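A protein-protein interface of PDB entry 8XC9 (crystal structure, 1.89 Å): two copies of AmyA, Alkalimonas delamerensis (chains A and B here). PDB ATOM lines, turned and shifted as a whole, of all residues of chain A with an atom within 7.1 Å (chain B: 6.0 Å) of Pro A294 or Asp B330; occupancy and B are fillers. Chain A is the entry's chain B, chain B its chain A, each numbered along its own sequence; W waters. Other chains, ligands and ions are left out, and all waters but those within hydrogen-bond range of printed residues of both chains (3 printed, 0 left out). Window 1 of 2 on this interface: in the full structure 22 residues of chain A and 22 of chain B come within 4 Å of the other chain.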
ATOM      1  N   ILE A 262      -2.352  -8.618  -1.882  1.00  0.00           N
ATOM      2  CA  ILE A 262      -2.475 -10.054  -2.112  1.00  0.00           C
ATOM      3  C   ILE A 262      -3.557 -10.326  -3.146  1.00  0.00           C
ATOM      4  O   ILE A 262      -3.354 -11.068  -4.116  1.00  0.00           O
ATOM      5  CB  ILE A 262      -2.786 -10.779  -0.796  1.00  0.00           C
ATOM      6  CG1 ILE A 262      -1.599 -10.692   0.162  1.00  0.00           C
ATOM      7  CG2 ILE A 262      -3.220 -12.215  -1.090  1.00  0.00           C
ATOM      8  CD1 ILE A 262      -1.836 -11.425   1.481  1.00  0.00           C
ATOM      9  N   ASN A 263      -4.731  -9.741  -2.936  1.00  0.00           N
ATOM     10  CA  ASN A 263      -5.851 -10.010  -3.839  1.00  0.00           C
ATOM     11  C   ASN A 263      -5.524  -9.577  -5.259  1.00  0.00           C
ATOM     12  O   ASN A 263      -5.892 -10.259  -6.223  1.00  0.00           O
ATOM     13  CB  ASN A 263      -7.114  -9.308  -3.339  1.00  0.00           C
ATOM     14  CG  ASN A 263      -8.392  -9.919  -3.913  1.00  0.00           C
ATOM     15  OD1 ASN A 263      -8.543 -11.139  -3.976  1.00  0.00           O
ATOM     16  ND2 ASN A 263      -9.302  -9.066  -4.352  1.00  0.00           N
ATOM     17  N   GLN A 266      -2.860 -12.010  -6.860  1.00  0.00           N
ATOM     18  CA  GLN A 266      -3.457 -13.305  -7.169  1.00  0.00           C
ATOM     19  C   GLN A 266      -4.298 -13.213  -8.436  1.00  0.00           C
ATOM     20  O   GLN A 266      -4.081 -13.952  -9.403  1.00  0.00           O
ATOM     21  CB  GLN A 266      -4.295 -13.789  -5.985  1.00  0.00           C
ATOM     22  CG  GLN A 266      -4.734 -15.257  -6.084  1.00  0.00           C
ATOM     23  CD  GLN A 266      -3.565 -16.219  -6.037  1.00  0.00           C
ATOM     24  OE1 GLN A 266      -2.850 -16.398  -7.031  1.00  0.00           O
ATOM     25  NE2 GLN A 266      -3.356 -16.848  -4.869  1.00  0.00           N
ATOM     26  N   VAL A 291      -7.087  -9.596   8.095  1.00  0.00           N
ATOM     27  CA  VAL A 291      -6.712  -9.453   6.690  1.00  0.00           C
ATOM     28  C   VAL A 291      -7.827  -9.982   5.797  1.00  0.00           C
ATOM     29  O   VAL A 291      -8.229  -9.329   4.829  1.00  0.00           O
ATOM     30  CB  VAL A 291      -5.380 -10.161   6.396  1.00  0.00           C
ATOM     31  CG1 VAL A 291      -5.077 -10.115   4.923  1.00  0.00           C
ATOM     32  CG2 VAL A 291      -4.222  -9.489   7.160  1.00  0.00           C
ATOM     33  N   ASN A 292      -8.339 -11.179   6.112  1.00  0.00           N
ATOM     34  CA  ASN A 292      -9.548 -11.715   5.469  1.00  0.00           C
ATOM     35  C   ASN A 292      -9.364 -11.966   3.972  1.00  0.00           C
ATOM     36  O   ASN A 292     -10.176 -11.536   3.146  1.00  0.00           O
ATOM     37  CB  ASN A 292     -10.761 -10.801   5.716  1.00  0.00           C
ATOM     38  CG  ASN A 292     -12.101 -11.543   5.565  1.00  0.00           C
ATOM     39  OD1 ASN A 292     -12.136 -12.771   5.489  1.00  0.00           O
ATOM     40  ND2 ASN A 292     -13.200 -10.793   5.536  1.00  0.00           N
ATOM     41  N   THR A 293      -8.322 -12.720   3.622  1.00  0.00           N
ATOM     42  CA  THR A 293      -8.146 -13.271   2.276  1.00  0.00           C
ATOM     43  C   THR A 293      -7.832 -14.755   2.374  1.00  0.00           C
ATOM     44  O   THR A 293      -6.955 -15.156   3.159  1.00  0.00           O
ATOM     45  CB  THR A 293      -7.056 -12.553   1.466  1.00  0.00           C
ATOM     46  OG1 THR A 293      -6.872 -13.244   0.218  1.00  0.00           O
ATOM     47  CG2 THR A 293      -5.717 -12.458   2.250  1.00  0.00           C
ATOM     48  N   PRO A 294      -8.515 -15.605   1.599  1.00  0.00           N
ATOM     49  CA  PRO A 294      -8.238 -17.051   1.659  1.00  0.00           C
ATOM     50  C   PRO A 294      -6.837 -17.430   1.194  1.00  0.00           C
ATOM     51  O   PRO A 294      -6.402 -18.550   1.476  1.00  0.00           O
ATOM     52  CB  PRO A 294      -9.317 -17.658   0.749  1.00  0.00           C
ATOM     53  CG  PRO A 294      -9.747 -16.504  -0.151  1.00  0.00           C
ATOM     54  CD  PRO A 294      -9.637 -15.279   0.699  1.00  0.00           C
ATOM     55  N   HIS A 295      -6.105 -16.530   0.540  1.00  0.00           N
ATOM     56  CA  HIS A 295      -4.788 -16.843   0.001  1.00  0.00           C
ATOM     57  C   HIS A 295      -3.666 -16.693   1.014  1.00  0.00           C
ATOM     58  O   HIS A 295      -2.531 -17.054   0.694  1.00  0.00           O
ATOM     59  CB  HIS A 295      -4.449 -15.941  -1.188  1.00  0.00           C
ATOM     60  CG  HIS A 295      -5.575 -15.774  -2.151  1.00  0.00           C
ATOM     61  ND1 HIS A 295      -6.159 -16.842  -2.801  1.00  0.00           N
ATOM     62  CD2 HIS A 295      -6.239 -14.670  -2.564  1.00  0.00           C
ATOM     63  CE1 HIS A 295      -7.134 -16.401  -3.574  1.00  0.00           C
ATOM     64  NE2 HIS A 295      -7.203 -15.087  -3.449  1.00  0.00           N
ATOM     65  N   LEU A 296      -3.929 -16.142   2.191  1.00  0.00           N
ATOM     66  CA  LEU A 296      -2.866 -15.830   3.140  1.00  0.00           C
ATOM     67  C   LEU A 296      -2.722 -16.958   4.152  1.00  0.00           C
ATOM     68  O   LEU A 296      -3.677 -17.291   4.856  1.00  0.00           O
ATOM     69  CB  LEU A 296      -3.132 -14.523   3.874  1.00  0.00           C
ATOM     70  CG  LEU A 296      -1.957 -14.043   4.710  1.00  0.00           C
ATOM     71  CD1 LEU A 296      -0.677 -13.983   3.874  1.00  0.00           C
ATOM     72  CD2 LEU A 296      -2.288 -12.694   5.318  1.00  0.00           C
ATOM     73  N   ARG A 297      -1.524 -17.510   4.236  1.00  0.00           N
ATOM     74  CA  ARG A 297      -1.136 -18.428   5.294  1.00  0.00           C
ATOM     75  C   ARG A 297      -0.283 -17.684   6.325  1.00  0.00           C
ATOM     76  O   ARG A 297       0.072 -16.519   6.142  1.00  0.00           O
ATOM     77  CB  ARG A 297      -0.382 -19.607   4.686  1.00  0.00           C
ATOM     78  CG  ARG A 297      -1.151 -20.355   3.604  1.00  0.00           C
ATOM     79  CD  ARG A 297      -0.209 -21.138   2.696  1.00  0.00           C
ATOM     80  NE  ARG A 297      -0.817 -21.502   1.410  1.00  0.00           N
ATOM     81  CZ  ARG A 297      -1.340 -22.697   1.134  1.00  0.00           C
ATOM     82  NH1 ARG A 297      -1.355 -23.657   2.055  1.00  0.00           N
ATOM     83  NH2 ARG A 297      -1.850 -22.934  -0.063  1.00  0.00           N
ATOM     84  N   ASP A 330      -5.497 -25.213   8.287  1.00  0.00           N
ATOM     85  CA  ASP A 330      -5.257 -25.258   6.846  1.00  0.00           C
ATOM     86  C   ASP A 330      -4.378 -24.110   6.362  1.00  0.00           C
ATOM     87  O   ASP A 330      -3.711 -24.233   5.327  1.00  0.00           O
ATOM     88  CB  ASP A 330      -6.598 -25.218   6.089  1.00  0.00           C
ATOM     89  CG  ASP A 330      -7.520 -24.090   6.581  1.00  0.00           C
ATOM     90  OD1 ASP A 330      -7.934 -24.123   7.769  1.00  0.00           O
ATOM     91  OD2 ASP A 330      -7.830 -23.164   5.785  1.00  0.00           O
ATOM     92  N   ARG A 331      -4.370 -22.989   7.073  1.00  0.00           N
ATOM     93  CA  ARG A 331      -3.589 -21.838   6.654  1.00  0.00           C
ATOM     94  C   ARG A 331      -2.279 -21.728   7.427  1.00  0.00           C
ATOM     95  O   ARG A 331      -1.652 -20.665   7.434  1.00  0.00           O
ATOM     96  CB  ARG A 331      -4.436 -20.568   6.787  1.00  0.00           C
ATOM     97  CG  ARG A 331      -5.383 -20.316   5.582  1.00  0.00           C
ATOM     98  CD  ARG A 331      -6.672 -19.578   5.976  1.00  0.00           C
ATOM     99  NE  ARG A 331      -7.613 -20.435   6.709  1.00  0.00           N
ATOM    100  CZ  ARG A 331      -8.678 -19.992   7.379  1.00  0.00           C
ATOM    101  NH1 ARG A 331      -8.948 -18.691   7.400  1.00  0.00           N
ATOM    102  NH2 ARG A 331      -9.470 -20.847   8.026  1.00  0.00           N
ATOM    103  N   ARG B 297     -18.384 -25.110   2.840  1.00  0.00           N
ATOM    104  CA  ARG B 297     -19.048 -23.823   2.747  1.00  0.00           C
ATOM    105  C   ARG B 297     -20.355 -23.864   3.533  1.00  0.00           C
ATOM    106  O   ARG B 297     -20.791 -24.923   3.998  1.00  0.00           O
ATOM    107  CB  ARG B 297     -19.294 -23.488   1.285  1.00  0.00           C
ATOM    108  CG  ARG B 297     -18.060 -23.721   0.442  1.00  0.00           C
ATOM    109  CD  ARG B 297     -18.351 -23.597  -1.017  1.00  0.00           C
ATOM    110  NE  ARG B 297     -17.225 -24.013  -1.847  1.00  0.00           N
ATOM    111  CZ  ARG B 297     -16.487 -23.171  -2.566  1.00  0.00           C
ATOM    112  NH1 ARG B 297     -16.750 -21.861  -2.555  1.00  0.00           N
ATOM    113  NH2 ARG B 297     -15.482 -23.637  -3.295  1.00  0.00           N
ATOM    114  N   LEU B 323     -22.777 -13.364   6.223  1.00  0.00           N
ATOM    115  CA  LEU B 323     -21.555 -14.162   6.175  1.00  0.00           C
ATOM    116  C   LEU B 323     -20.653 -13.729   5.027  1.00  0.00           C
ATOM    117  O   LEU B 323     -19.418 -13.770   5.151  1.00  0.00           O
ATOM    118  CB  LEU B 323     -21.920 -15.642   6.041  1.00  0.00           C
ATOM    119  CG  LEU B 323     -20.807 -16.681   6.118  1.00  0.00           C
ATOM    120  CD1 LEU B 323     -20.229 -16.697   7.509  1.00  0.00           C
ATOM    121  CD2 LEU B 323     -21.388 -18.068   5.752  1.00  0.00           C
ATOM    122  N   SER B 326     -18.239 -11.290   6.209  1.00  0.00           N
ATOM    123  CA  SER B 326     -17.555 -11.692   7.431  1.00  0.00           C
ATOM    124  C   SER B 326     -16.157 -12.216   7.123  1.00  0.00           C
ATOM    125  O   SER B 326     -15.714 -12.243   5.974  1.00  0.00           O
ATOM    126  CB  SER B 326     -18.374 -12.779   8.141  1.00  0.00           C
ATOM    127  OG  SER B 326     -18.168 -14.014   7.483  1.00  0.00           O
ATOM    128  N   GLN B 327     -15.476 -12.699   8.181  1.00  0.00           N
ATOM    129  CA  GLN B 327     -14.196 -13.400   8.088  1.00  0.00           C
ATOM    130  C   GLN B 327     -14.296 -14.773   7.425  1.00  0.00           C
ATOM    131  O   GLN B 327     -13.258 -15.337   7.060  1.00  0.00           O
ATOM    132  CB  GLN B 327     -13.582 -13.567   9.484  1.00  0.00           C
ATOM    133  CG  GLN B 327     -14.302 -14.577  10.392  1.00  0.00           C
ATOM    134  CD  GLN B 327     -15.398 -13.925  11.227  1.00  0.00           C
ATOM    135  OE1 GLN B 327     -15.936 -12.881  10.858  1.00  0.00           O
ATOM    136  NE2 GLN B 327     -15.727 -14.531  12.354  1.00  0.00           N
ATOM    137  N   HIS B 328     -15.503 -15.323   7.259  1.00  0.00           N
ATOM    138  CA  HIS B 328     -15.720 -16.546   6.495  1.00  0.00           C
ATOM    139  C   HIS B 328     -16.352 -16.280   5.127  1.00  0.00           C
ATOM    140  O   HIS B 328     -16.974 -17.174   4.549  1.00  0.00           O
ATOM    141  CB  HIS B 328     -16.592 -17.526   7.283  1.00  0.00           C
ATOM    142  CG  HIS B 328     -15.938 -18.082   8.511  1.00  0.00           C
ATOM    143  ND1 HIS B 328     -16.039 -17.475   9.744  1.00  0.00           N
ATOM    144  CD2 HIS B 328     -15.195 -19.200   8.703  1.00  0.00           C
ATOM    145  CE1 HIS B 328     -15.385 -18.192  10.642  1.00  0.00           C
ATOM    146  NE2 HIS B 328     -14.862 -19.241  10.033  1.00  0.00           N
ATOM    147  N   ARG B 329     -16.163 -15.069   4.578  1.00  0.00           N
ATOM    148  CA  ARG B 329     -16.798 -14.710   3.311  1.00  0.00           C
ATOM    149  C   ARG B 329     -16.448 -15.697   2.204  1.00  0.00           C
ATOM    150  O   ARG B 329     -17.305 -16.055   1.391  1.00  0.00           O
ATOM    151  CB  ARG B 329     -16.381 -13.291   2.894  1.00  0.00           C
ATOM    152  CG  ARG B 329     -14.878 -13.061   3.019  1.00  0.00           C
ATOM    153  CD  ARG B 329     -14.368 -11.937   2.141  1.00  0.00           C
ATOM    154  NE  ARG B 329     -14.624 -10.635   2.733  1.00  0.00           N
ATOM    155  CZ  ARG B 329     -13.817  -9.579   2.644  1.00  0.00           C
ATOM    156  NH1 ARG B 329     -12.657  -9.649   1.999  1.00  0.00           N
ATOM    157  NH2 ARG B 329     -14.186  -8.446   3.217  1.00  0.00           N
ATOM    158  N   ASP B 330     -15.197 -16.147   2.147  1.00  0.00           N
ATOM    159  CA  ASP B 330     -14.799 -17.045   1.069  1.00  0.00           C
ATOM    160  C   ASP B 330     -15.516 -18.396   1.132  1.00  0.00           C
ATOM    161  O   ASP B 330     -15.415 -19.176   0.176  1.00  0.00           O
ATOM    162  CB  ASP B 330     -13.301 -17.288   1.121  1.00  0.00           C
ATOM    163  CG  ASP B 330     -12.883 -18.003   2.400  1.00  0.00           C
ATOM    164  OD1 ASP B 330     -12.992 -17.383   3.493  1.00  0.00           O
ATOM    165  OD2 ASP B 330     -12.469 -19.184   2.317  1.00  0.00           O
ATOM    166  N   ARG B 331     -16.183 -18.703   2.244  1.00  0.00           N
ATOM    167  CA  ARG B 331     -16.935 -19.948   2.396  1.00  0.00           C
ATOM    168  C   ARG B 331     -18.440 -19.712   2.389  1.00  0.00           C
ATOM    169  O   ARG B 331     -19.212 -20.617   2.732  1.00  0.00           O
ATOM    170  CB  ARG B 331     -16.498 -20.661   3.674  1.00  0.00           C
ATOM    171  CG  ARG B 331     -15.145 -21.365   3.545  1.00  0.00           C
ATOM    172  CD  ARG B 331     -14.390 -21.333   4.868  1.00  0.00           C
ATOM    173  NE  ARG B 331     -13.590 -20.113   4.982  1.00  0.00           N
ATOM    174  CZ  ARG B 331     -12.924 -19.738   6.074  1.00  0.00           C
ATOM    175  NH1 ARG B 331     -12.954 -20.490   7.169  1.00  0.00           N
ATOM    176  NH2 ARG B 331     -12.225 -18.603   6.067  1.00  0.00           N
ATOM    177  N   ALA B 332     -18.882 -18.520   1.987  1.00  0.00           N
ATOM    178  CA  ALA B 332     -20.307 -18.230   1.932  1.00  0.00           C
ATOM    179  C   ALA B 332     -20.909 -18.766   0.640  1.00  0.00           C
ATOM    180  O   ALA B 332     -20.268 -18.740  -0.414  1.00  0.00           O
ATOM    181  CB  ALA B 332     -20.541 -16.724   2.059  1.00  0.00           C
ATOM    182  N   HIS B 369     -16.926 -12.108  -3.451  1.00  0.00           N
ATOM    183  CA  HIS B 369     -16.875 -13.228  -2.520  1.00  0.00           C
ATOM    184  C   HIS B 369     -18.172 -14.025  -2.561  1.00  0.00           C
ATOM    185  O   HIS B 369     -19.230 -13.522  -2.942  1.00  0.00           O
ATOM    186  CB  HIS B 369     -16.613 -12.735  -1.098  1.00  0.00           C
ATOM    187  CG  HIS B 369     -15.604 -11.635  -1.037  1.00  0.00           C
ATOM    188  ND1 HIS B 369     -14.250 -11.865  -1.151  1.00  0.00           N
ATOM    189  CD2 HIS B 369     -15.754 -10.295  -0.920  1.00  0.00           C
ATOM    190  CE1 HIS B 369     -13.607 -10.713  -1.081  1.00  0.00           C
ATOM    191  NE2 HIS B 369     -14.498  -9.743  -0.952  1.00  0.00           N
ATOM    192  N   GLY B 370     -18.076 -15.283  -2.155  1.00  0.00           N
ATOM    193  CA  GLY B 370     -19.231 -16.149  -2.113  1.00  0.00           C
ATOM    194  C   GLY B 370     -19.500 -16.839  -3.439  1.00  0.00           C
ATOM    195  O   GLY B 370     -18.986 -16.463  -4.493  1.00  0.00           O
HETATM  196  O   HOH W   1     -10.437 -14.892   6.939  1.00  0.00           O
HETATM  197  O   HOH W   2     -10.551 -10.937   0.116  1.00  0.00           O
HETATM  198  O   HOH W   3     -12.713  -7.980   6.120  1.00  0.00           O
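The backbone carbonyl oxygen (O) of Ser B326 is in hydrogen-bond range of the side-chain amide nitrogen (ND2) of Asn A292, at 2.9 Å.
NE of Arg B329 sits close to ND2 of Asn A292 (3.1 Å).
OD1 of Asn A292 lies close to O of Gln B327 (3.2 Å).
Pro A294 touches Asp B330 (CB to OD2, 3.8 Å).
Arg B331 touches Arg A331.
Water W1 bridges the backbone carbonyl oxygen of Gln B327 (2.9 Å) and the side-chain amide oxygen of Asn A292 (3.1 Å).
Water W3 lies within hydrogen-bond range of the side-chain amide nitrogen of Asn A292 and the guanidinium group of Arg B329.
Water W2 bridges NH1 of Arg B329 and O of Asn A292.
Of the 12 printed residues of chain A, 3 touch a printed residue of chain B.
Printed residues of chain A that touch a printed residue of chain B: Asn A292, Pro A294 and Arg A331.
Hydrophobic or aromatic side chains of chain A within 4 Å of the printed part of chain B: Pro A294.
Printed residues of chain B that touch a printed residue of chain A: Ser B326, Gln B327, Arg B329, Asp B330 and Arg B331.
Among the printed residues, no Asp or Glu carboxylate lies within 4 Å of a Lys or Arg side-chain nitrogen of the other chain.
Printed residues of chain B within 4 Å of Pro A294: Asp B330 (3.8 Å).
Asp B330 touches one residue of chain A.
Of the printed residues of chain A, Ser B326 touches Asn A292.
Of the printed residues of chain B, Asn A292 touches Ser B326, Gln B327 and Arg B329.
Of the printed residues of chain A, Arg B331 touches Arg A331 (3.5 Å).
Printed residues of chain B within 4 Å of Arg A331: Arg B331.
Printed residues of chain A within 4 Å of Gln B327: Asn A292 (3.2 Å).
Asn A263 touches none of the printed residues of chain B.
Leu A296 touches none of the printed residues of chain B.
Arg B331 touches its own counterpart, Arg A331.
Positions printed for both chains: 297, 330 and 331.
A ring nitrogen (NE2) of His B369 lies close to the guanidinium group of Arg B329 (3.5 Å).
OG of Ser B326 sits at hydrogen-bond distance from O of Leu B323 (2.7 Å).
NE of Arg A331 is in salt-bridge range of OD2 of Asp A330 (2.9 Å).
The side-chain carboxylate of Asp B330 is in salt-bridge range of the guanidinium group of Arg B331 (2.9 Å).
The side-chain hydroxyl (OG) of Ser B326 sits at hydrogen-bond distance from the backbone NH (N) of His B328.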
